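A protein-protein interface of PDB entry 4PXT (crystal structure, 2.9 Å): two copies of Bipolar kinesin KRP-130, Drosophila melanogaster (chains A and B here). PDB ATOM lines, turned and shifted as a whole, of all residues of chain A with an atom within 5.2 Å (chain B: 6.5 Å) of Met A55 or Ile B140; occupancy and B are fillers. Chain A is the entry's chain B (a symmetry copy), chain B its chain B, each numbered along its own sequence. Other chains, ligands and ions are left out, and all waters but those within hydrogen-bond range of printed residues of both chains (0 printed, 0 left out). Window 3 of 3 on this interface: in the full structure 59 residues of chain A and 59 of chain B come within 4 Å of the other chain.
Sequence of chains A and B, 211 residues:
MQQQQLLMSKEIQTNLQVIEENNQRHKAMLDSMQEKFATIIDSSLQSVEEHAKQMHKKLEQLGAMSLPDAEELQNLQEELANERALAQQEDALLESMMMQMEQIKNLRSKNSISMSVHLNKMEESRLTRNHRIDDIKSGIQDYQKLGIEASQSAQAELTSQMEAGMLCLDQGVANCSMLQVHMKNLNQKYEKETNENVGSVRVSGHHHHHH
NE2 of His A51 lies close to SD of Met A55 (3.7 Å).
Among the printed residues, merely in contact across the chains: His A51 with Tyr B143 (3.5 Å), Met A55 with Ile B140 (3.6 Å), Met A55 with Ile B136 (3.9 Å), Lys A58 with Asp B135 (3.9 Å) and Leu A59 with Ile B136 (3.98 Å).
Ile B140 touches one residue of chain A.
Of the printed residues of chain A, Tyr B143 touches His A51.
Printed residues of chain A within 4 Å of Asp B135: Lys A58 (3.9 Å).
Of the printed residues of chain B, His A51 touches Tyr B143 (3.5 Å).
Of the printed residues of chain B, Lys A58 touches Asp B135.
Of the printed residues of chain B, Leu A59 touches Ile B136 (3.98 Å).
The nearest residue of chain A that does not touch Ile B140 is His A51 (4.2 Å).
The nearest printed residue of chain A that does not touch Ile B136 is Lys A58 (4.1 Å).
Printed residues of chain B that touch a printed residue of chain A: Asp B135, Ile B136, Ile B140 and Tyr B143.
Hydrophobic or aromatic side chains of chain A that line the printed part of chain B: His A51, Met A55 and Leu A59.
Among the printed residues, 5 pairs touch across the chains.
Among the printed residues, no Asp or Glu carboxylate lies within 4 Å of a Lys or Arg side-chain nitrogen of the other chain.
No position is printed for both chains.
Of the 5 pairs that touch across the chains among the printed residues, none has its exchanged pair printed and touching as well.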
ATOM      1  N   HIS A  51       8.850  28.995 -26.092  1.00  0.00           N
ATOM      2  CA  HIS A  51       7.973  28.132 -26.875  1.00  0.00           C
ATOM      3  C   HIS A  51       8.006  26.708 -26.337  1.00  0.00           C
ATOM      4  O   HIS A  51       6.968  26.060 -26.230  1.00  0.00           O
ATOM      5  CB  HIS A  51       8.381  28.173 -28.348  1.00  0.00           C
ATOM      6  CG  HIS A  51       7.691  27.160 -29.209  1.00  0.00           C
ATOM      7  ND1 HIS A  51       8.315  26.013 -29.654  1.00  0.00           N
ATOM      8  CD2 HIS A  51       6.444  27.137 -29.737  1.00  0.00           C
ATOM      9  CE1 HIS A  51       7.479  25.323 -30.410  1.00  0.00           C
ATOM     10  NE2 HIS A  51       6.338  25.984 -30.480  1.00  0.00           N
ATOM     11  N   ALA A  52       9.198  26.229 -25.989  1.00  0.00           N
ATOM     12  CA  ALA A  52       9.362  24.879 -25.446  1.00  0.00           C
ATOM     13  C   ALA A  52       8.573  24.709 -24.147  1.00  0.00           C
ATOM     14  O   ALA A  52       8.071  23.627 -23.848  1.00  0.00           O
ATOM     15  CB  ALA A  52      10.839  24.575 -25.213  1.00  0.00           C
ATOM     16  N   LYS A  53       8.468  25.795 -23.391  1.00  0.00           N
ATOM     17  CA  LYS A  53       7.666  25.835 -22.174  1.00  0.00           C
ATOM     18  C   LYS A  53       6.167  25.731 -22.460  1.00  0.00           C
ATOM     19  O   LYS A  53       5.461  24.950 -21.829  1.00  0.00           O
ATOM     20  CB  LYS A  53       7.966  27.120 -21.406  1.00  0.00           C
ATOM     21  CG  LYS A  53       7.106  27.363 -20.184  1.00  0.00           C
ATOM     22  CD  LYS A  53       7.164  28.833 -19.798  1.00  0.00           C
ATOM     23  CE  LYS A  53       8.607  29.325 -19.738  1.00  0.00           C
ATOM     24  NZ  LYS A  53       8.702  30.813 -19.642  1.00  0.00           N
ATOM     25  N   GLN A  54       5.695  26.513 -23.426  1.00  0.00           N
ATOM     26  CA  GLN A  54       4.269  26.605 -23.736  1.00  0.00           C
ATOM     27  C   GLN A  54       3.735  25.325 -24.371  1.00  0.00           C
ATOM     28  O   GLN A  54       2.565  24.961 -24.201  1.00  0.00           O
ATOM     29  CB  GLN A  54       4.007  27.799 -24.660  1.00  0.00           C
ATOM     30  CG  GLN A  54       2.548  27.992 -25.047  1.00  0.00           C
ATOM     31  CD  GLN A  54       1.653  28.276 -23.855  1.00  0.00           C
ATOM     32  OE1 GLN A  54       2.087  28.860 -22.861  1.00  0.00           O
ATOM     33  NE2 GLN A  54       0.396  27.844 -23.942  1.00  0.00           N
ATOM     34  N   MET A  55       4.601  24.636 -25.099  1.00  0.00           N
ATOM     35  CA  MET A  55       4.207  23.413 -25.779  1.00  0.00           C
ATOM     36  C   MET A  55       4.217  22.212 -24.859  1.00  0.00           C
ATOM     37  O   MET A  55       3.205  21.526 -24.720  1.00  0.00           O
ATOM     38  CB  MET A  55       5.115  23.163 -26.966  1.00  0.00           C
ATOM     39  CG  MET A  55       4.986  24.242 -27.995  1.00  0.00           C
ATOM     40  SD  MET A  55       3.639  23.757 -29.299  1.00  0.00           S
ATOM     41  CE  MET A  55       4.665  22.337 -30.186  1.00  0.00           C
ATOM     42  N   HIS A  56       5.363  21.954 -24.238  1.00  0.00           N
ATOM     43  CA  HIS A  56       5.485  20.847 -23.302  1.00  0.00           C
ATOM     44  C   HIS A  56       4.374  20.907 -22.246  1.00  0.00           C
ATOM     45  O   HIS A  56       3.967  19.884 -21.707  1.00  0.00           O
ATOM     46  CB  HIS A  56       6.865  20.856 -22.641  1.00  0.00           C
ATOM     47  CG  HIS A  56       6.987  19.910 -21.488  1.00  0.00           C
ATOM     48  ND1 HIS A  56       6.855  20.311 -20.175  1.00  0.00           N
ATOM     49  CD2 HIS A  56       7.225  18.578 -21.451  1.00  0.00           C
ATOM     50  CE1 HIS A  56       7.009  19.268 -19.380  1.00  0.00           C
ATOM     51  NE2 HIS A  56       7.234  18.203 -20.129  1.00  0.00           N
ATOM     52  N   LYS A  57       3.882  22.111 -21.969  1.00  0.00           N
ATOM     53  CA  LYS A  57       2.722  22.294 -21.105  1.00  0.00           C
ATOM     54  C   LYS A  57       1.474  21.673 -21.718  1.00  0.00           C
ATOM     55  O   LYS A  57       0.795  20.873 -21.082  1.00  0.00           O
ATOM     56  CB  LYS A  57       2.478  23.779 -20.833  1.00  0.00           C
ATOM     57  CG  LYS A  57       1.182  24.072 -20.073  1.00  0.00           C
ATOM     58  CD  LYS A  57       1.168  25.505 -19.538  1.00  0.00           C
ATOM     59  CE  LYS A  57      -0.029  25.763 -18.629  1.00  0.00           C
ATOM     60  NZ  LYS A  57      -1.326  25.592 -19.340  1.00  0.00           N
ATOM     61  N   LYS A  58       1.179  22.047 -22.959  1.00  0.00           N
ATOM     62  CA  LYS A  58      -0.007  21.554 -23.650  1.00  0.00           C
ATOM     63  C   LYS A  58       0.132  20.093 -24.076  1.00  0.00           C
ATOM     64  O   LYS A  58      -0.866  19.416 -24.323  1.00  0.00           O
ATOM     65  CB  LYS A  58      -0.317  22.419 -24.869  1.00  0.00           C
ATOM     66  CG  LYS A  58      -1.014  23.721 -24.542  1.00  0.00           C
ATOM     67  CD  LYS A  58      -1.376  24.456 -25.822  1.00  0.00           C
ATOM     68  CE  LYS A  58      -2.085  25.768 -25.545  1.00  0.00           C
ATOM     69  NZ  LYS A  58      -2.407  26.479 -26.818  1.00  0.00           N
ATOM     70  N   LEU A  59       1.369  19.616 -24.166  1.00  0.00           N
ATOM     71  CA  LEU A  59       1.633  18.204 -24.444  1.00  0.00           C
ATOM     72  C   LEU A  59       1.413  17.335 -23.205  1.00  0.00           C
ATOM     73  O   LEU A  59       0.935  16.209 -23.309  1.00  0.00           O
ATOM     74  CB  LEU A  59       3.062  18.011 -24.954  1.00  0.00           C
ATOM     75  CG  LEU A  59       3.375  18.309 -26.418  1.00  0.00           C
ATOM     76  CD1 LEU A  59       4.760  17.783 -26.749  1.00  0.00           C
ATOM     77  CD2 LEU A  59       2.332  17.695 -27.333  1.00  0.00           C
ATOM     78  N   GLU A  60       1.783  17.848 -22.035  1.00  0.00           N
ATOM     79  CA  GLU A  60       1.613  17.097 -20.795  1.00  0.00           C
ATOM     80  C   GLU A  60       0.135  16.886 -20.486  1.00  0.00           C
ATOM     81  O   GLU A  60      -0.266  15.808 -20.051  1.00  0.00           O
ATOM     82  CB  GLU A  60       2.305  17.799 -19.624  1.00  0.00           C
ATOM     83  CG  GLU A  60       3.820  17.613 -19.589  1.00  0.00           C
ATOM     84  CD  GLU A  60       4.248  16.154 -19.520  1.00  0.00           C
ATOM     85  OE1 GLU A  60       3.438  15.305 -19.091  1.00  0.00           O
ATOM     86  OE2 GLU A  60       5.398  15.852 -19.906  1.00  0.00           O
ATOM     87  N   ASP B 135      -5.341  23.184 -31.593  1.00  0.00           N
ATOM     88  CA  ASP B 135      -4.775  24.388 -30.995  1.00  0.00           C
ATOM     89  C   ASP B 135      -3.265  24.325 -30.811  1.00  0.00           C
ATOM     90  O   ASP B 135      -2.635  25.348 -30.561  1.00  0.00           O
ATOM     91  CB  ASP B 135      -5.471  24.710 -29.657  1.00  0.00           C
ATOM     92  CG  ASP B 135      -5.040  23.804 -28.493  1.00  0.00           C
ATOM     93  OD1 ASP B 135      -3.952  23.188 -28.506  1.00  0.00           O
ATOM     94  OD2 ASP B 135      -5.819  23.727 -27.521  1.00  0.00           O
ATOM     95  N   ILE B 136      -2.689  23.127 -30.891  1.00  0.00           N
ATOM     96  CA  ILE B 136      -1.233  23.003 -30.850  1.00  0.00           C
ATOM     97  C   ILE B 136      -0.691  23.323 -32.243  1.00  0.00           C
ATOM     98  O   ILE B 136       0.389  23.902 -32.384  1.00  0.00           O
ATOM     99  CB  ILE B 136      -0.774  21.612 -30.380  1.00  0.00           C
ATOM    100  CG1 ILE B 136      -1.222  21.371 -28.940  1.00  0.00           C
ATOM    101  CG2 ILE B 136       0.736  21.498 -30.437  1.00  0.00           C
ATOM    102  CD1 ILE B 136      -0.682  20.095 -28.345  1.00  0.00           C
ATOM    103  N   LYS B 137      -1.455  22.955 -33.268  1.00  0.00           N
ATOM    104  CA  LYS B 137      -1.143  23.388 -34.621  1.00  0.00           C
ATOM    105  C   LYS B 137      -1.189  24.910 -34.682  1.00  0.00           C
ATOM    106  O   LYS B 137      -0.241  25.553 -35.147  1.00  0.00           O
ATOM    107  CB  LYS B 137      -2.117  22.795 -35.640  1.00  0.00           C
ATOM    108  CG  LYS B 137      -2.194  21.279 -35.652  1.00  0.00           C
ATOM    109  CD  LYS B 137      -3.198  20.806 -36.695  1.00  0.00           C
ATOM    110  CE  LYS B 137      -3.304  19.293 -36.738  1.00  0.00           C
ATOM    111  NZ  LYS B 137      -4.564  18.858 -37.416  1.00  0.00           N
ATOM    112  N   SER B 138      -2.288  25.478 -34.190  1.00  0.00           N
ATOM    113  CA  SER B 138      -2.460  26.924 -34.156  1.00  0.00           C
ATOM    114  C   SER B 138      -1.361  27.609 -33.339  1.00  0.00           C
ATOM    115  O   SER B 138      -0.913  28.701 -33.686  1.00  0.00           O
ATOM    116  CB  SER B 138      -3.838  27.274 -33.592  1.00  0.00           C
ATOM    117  OG  SER B 138      -3.877  28.591 -33.067  1.00  0.00           O
ATOM    118  N   GLY B 139      -0.922  26.959 -32.265  1.00  0.00           N
ATOM    119  CA  GLY B 139       0.138  27.487 -31.425  1.00  0.00           C
ATOM    120  C   GLY B 139       1.507  27.526 -32.086  1.00  0.00           C
ATOM    121  O   GLY B 139       2.354  28.368 -31.761  1.00  0.00           O
ATOM    122  N   ILE B 140       1.726  26.596 -33.007  1.00  0.00           N
ATOM    123  CA  ILE B 140       2.988  26.505 -33.723  1.00  0.00           C
ATOM    124  C   ILE B 140       3.012  27.529 -34.832  1.00  0.00           C
ATOM    125  O   ILE B 140       4.016  28.205 -35.059  1.00  0.00           O
ATOM    126  CB  ILE B 140       3.191  25.104 -34.289  1.00  0.00           C
ATOM    127  CG1 ILE B 140       3.736  24.194 -33.196  1.00  0.00           C
ATOM    128  CG2 ILE B 140       4.124  25.119 -35.495  1.00  0.00           C
ATOM    129  CD1 ILE B 140       3.763  22.767 -33.594  1.00  0.00           C
ATOM    130  N   GLN B 141       1.890  27.643 -35.522  1.00  0.00           N
ATOM    131  CA  GLN B 141       1.750  28.645 -36.555  1.00  0.00           C
ATOM    132  C   GLN B 141       1.921  30.040 -35.946  1.00  0.00           C
ATOM    133  O   GLN B 141       2.467  30.940 -36.578  1.00  0.00           O
ATOM    134  CB  GLN B 141       0.398  28.496 -37.238  1.00  0.00           C
ATOM    135  CG  GLN B 141       0.195  27.131 -37.866  1.00  0.00           C
ATOM    136  CD  GLN B 141      -1.153  26.992 -38.537  1.00  0.00           C
ATOM    137  OE1 GLN B 141      -2.188  27.352 -37.966  1.00  0.00           O
ATOM    138  NE2 GLN B 141      -1.154  26.463 -39.753  1.00  0.00           N
ATOM    139  N   ASP B 142       1.468  30.206 -34.707  1.00  0.00           N
ATOM    140  CA  ASP B 142       1.709  31.435 -33.968  1.00  0.00           C
ATOM    141  C   ASP B 142       3.204  31.645 -33.762  1.00  0.00           C
ATOM    142  O   ASP B 142       3.727  32.731 -34.006  1.00  0.00           O
ATOM    143  CB  ASP B 142       1.000  31.401 -32.611  1.00  0.00           C
ATOM    144  CG  ASP B 142      -0.496  31.595 -32.729  1.00  0.00           C
ATOM    145  OD1 ASP B 142      -0.945  32.111 -33.771  1.00  0.00           O
ATOM    146  OD2 ASP B 142      -1.223  31.231 -31.781  1.00  0.00           O
ATOM    147  N   TYR B 143       3.887  30.595 -33.325  1.00  0.00           N
ATOM    148  CA  TYR B 143       5.319  30.667 -33.081  1.00  0.00           C
ATOM    149  C   TYR B 143       6.070  30.997 -34.364  1.00  0.00           C
ATOM    150  O   TYR B 143       7.023  31.774 -34.357  1.00  0.00           O
ATOM    151  CB  TYR B 143       5.830  29.353 -32.490  1.00  0.00           C
ATOM    152  CG  TYR B 143       7.329  29.311 -32.301  1.00  0.00           C
ATOM    153  CD1 TYR B 143       7.957  30.161 -31.396  1.00  0.00           C
ATOM    154  CD2 TYR B 143       8.115  28.419 -33.020  1.00  0.00           C
ATOM    155  CE1 TYR B 143       9.330  30.128 -31.215  1.00  0.00           C
ATOM    156  CE2 TYR B 143       9.487  28.376 -32.847  1.00  0.00           C
ATOM    157  CZ  TYR B 143      10.091  29.234 -31.944  1.00  0.00           C
ATOM    158  OH  TYR B 143      11.460  29.202 -31.771  1.00  0.00           O
ATOM    159  N   GLN B 144       5.628  30.404 -35.466  1.00  0.00           N
ATOM    160  CA  GLN B 144       6.217  30.676 -36.768  1.00  0.00           C
ATOM    161  C   GLN B 144       6.008  32.138 -37.148  1.00  0.00           C
ATOM    162  O   GLN B 144       6.941  32.830 -37.542  1.00  0.00           O
ATOM    163  CB  GLN B 144       5.613  29.753 -37.824  1.00  0.00           C
ATOM    164  CG  GLN B 144       6.227  29.887 -39.204  1.00  0.00           C
ATOM    165  CD  GLN B 144       5.724  28.814 -40.152  1.00  0.00           C
ATOM    166  OE1 GLN B 144       4.766  28.097 -39.841  1.00  0.00           O
ATOM    167  NE2 GLN B 144       6.374  28.690 -41.309  1.00  0.00           N
ATOM    168  N   LYS B 145       4.768  32.590 -37.019  1.00  0.00           N
ATOM    169  CA  LYS B 145       4.396  33.968 -37.288  1.00  0.00           C
ATOM    170  C   LYS B 145       5.245  34.954 -36.478  1.00  0.00           C
ATOM    171  O   LYS B 145       5.713  35.960 -37.009  1.00  0.00           O
ATOM    172  CB  LYS B 145       2.910  34.153 -36.993  1.00  0.00           C
ATOM    173  CG  LYS B 145       2.322  35.493 -37.373  1.00  0.00           C
ATOM    174  CD  LYS B 145       0.938  35.641 -36.759  1.00  0.00           C
ATOM    175  CE  LYS B 145       0.180  34.312 -36.822  1.00  0.00           C
ATOM    176  NZ  LYS B 145      -0.941  34.215 -35.845  1.00  0.00           N
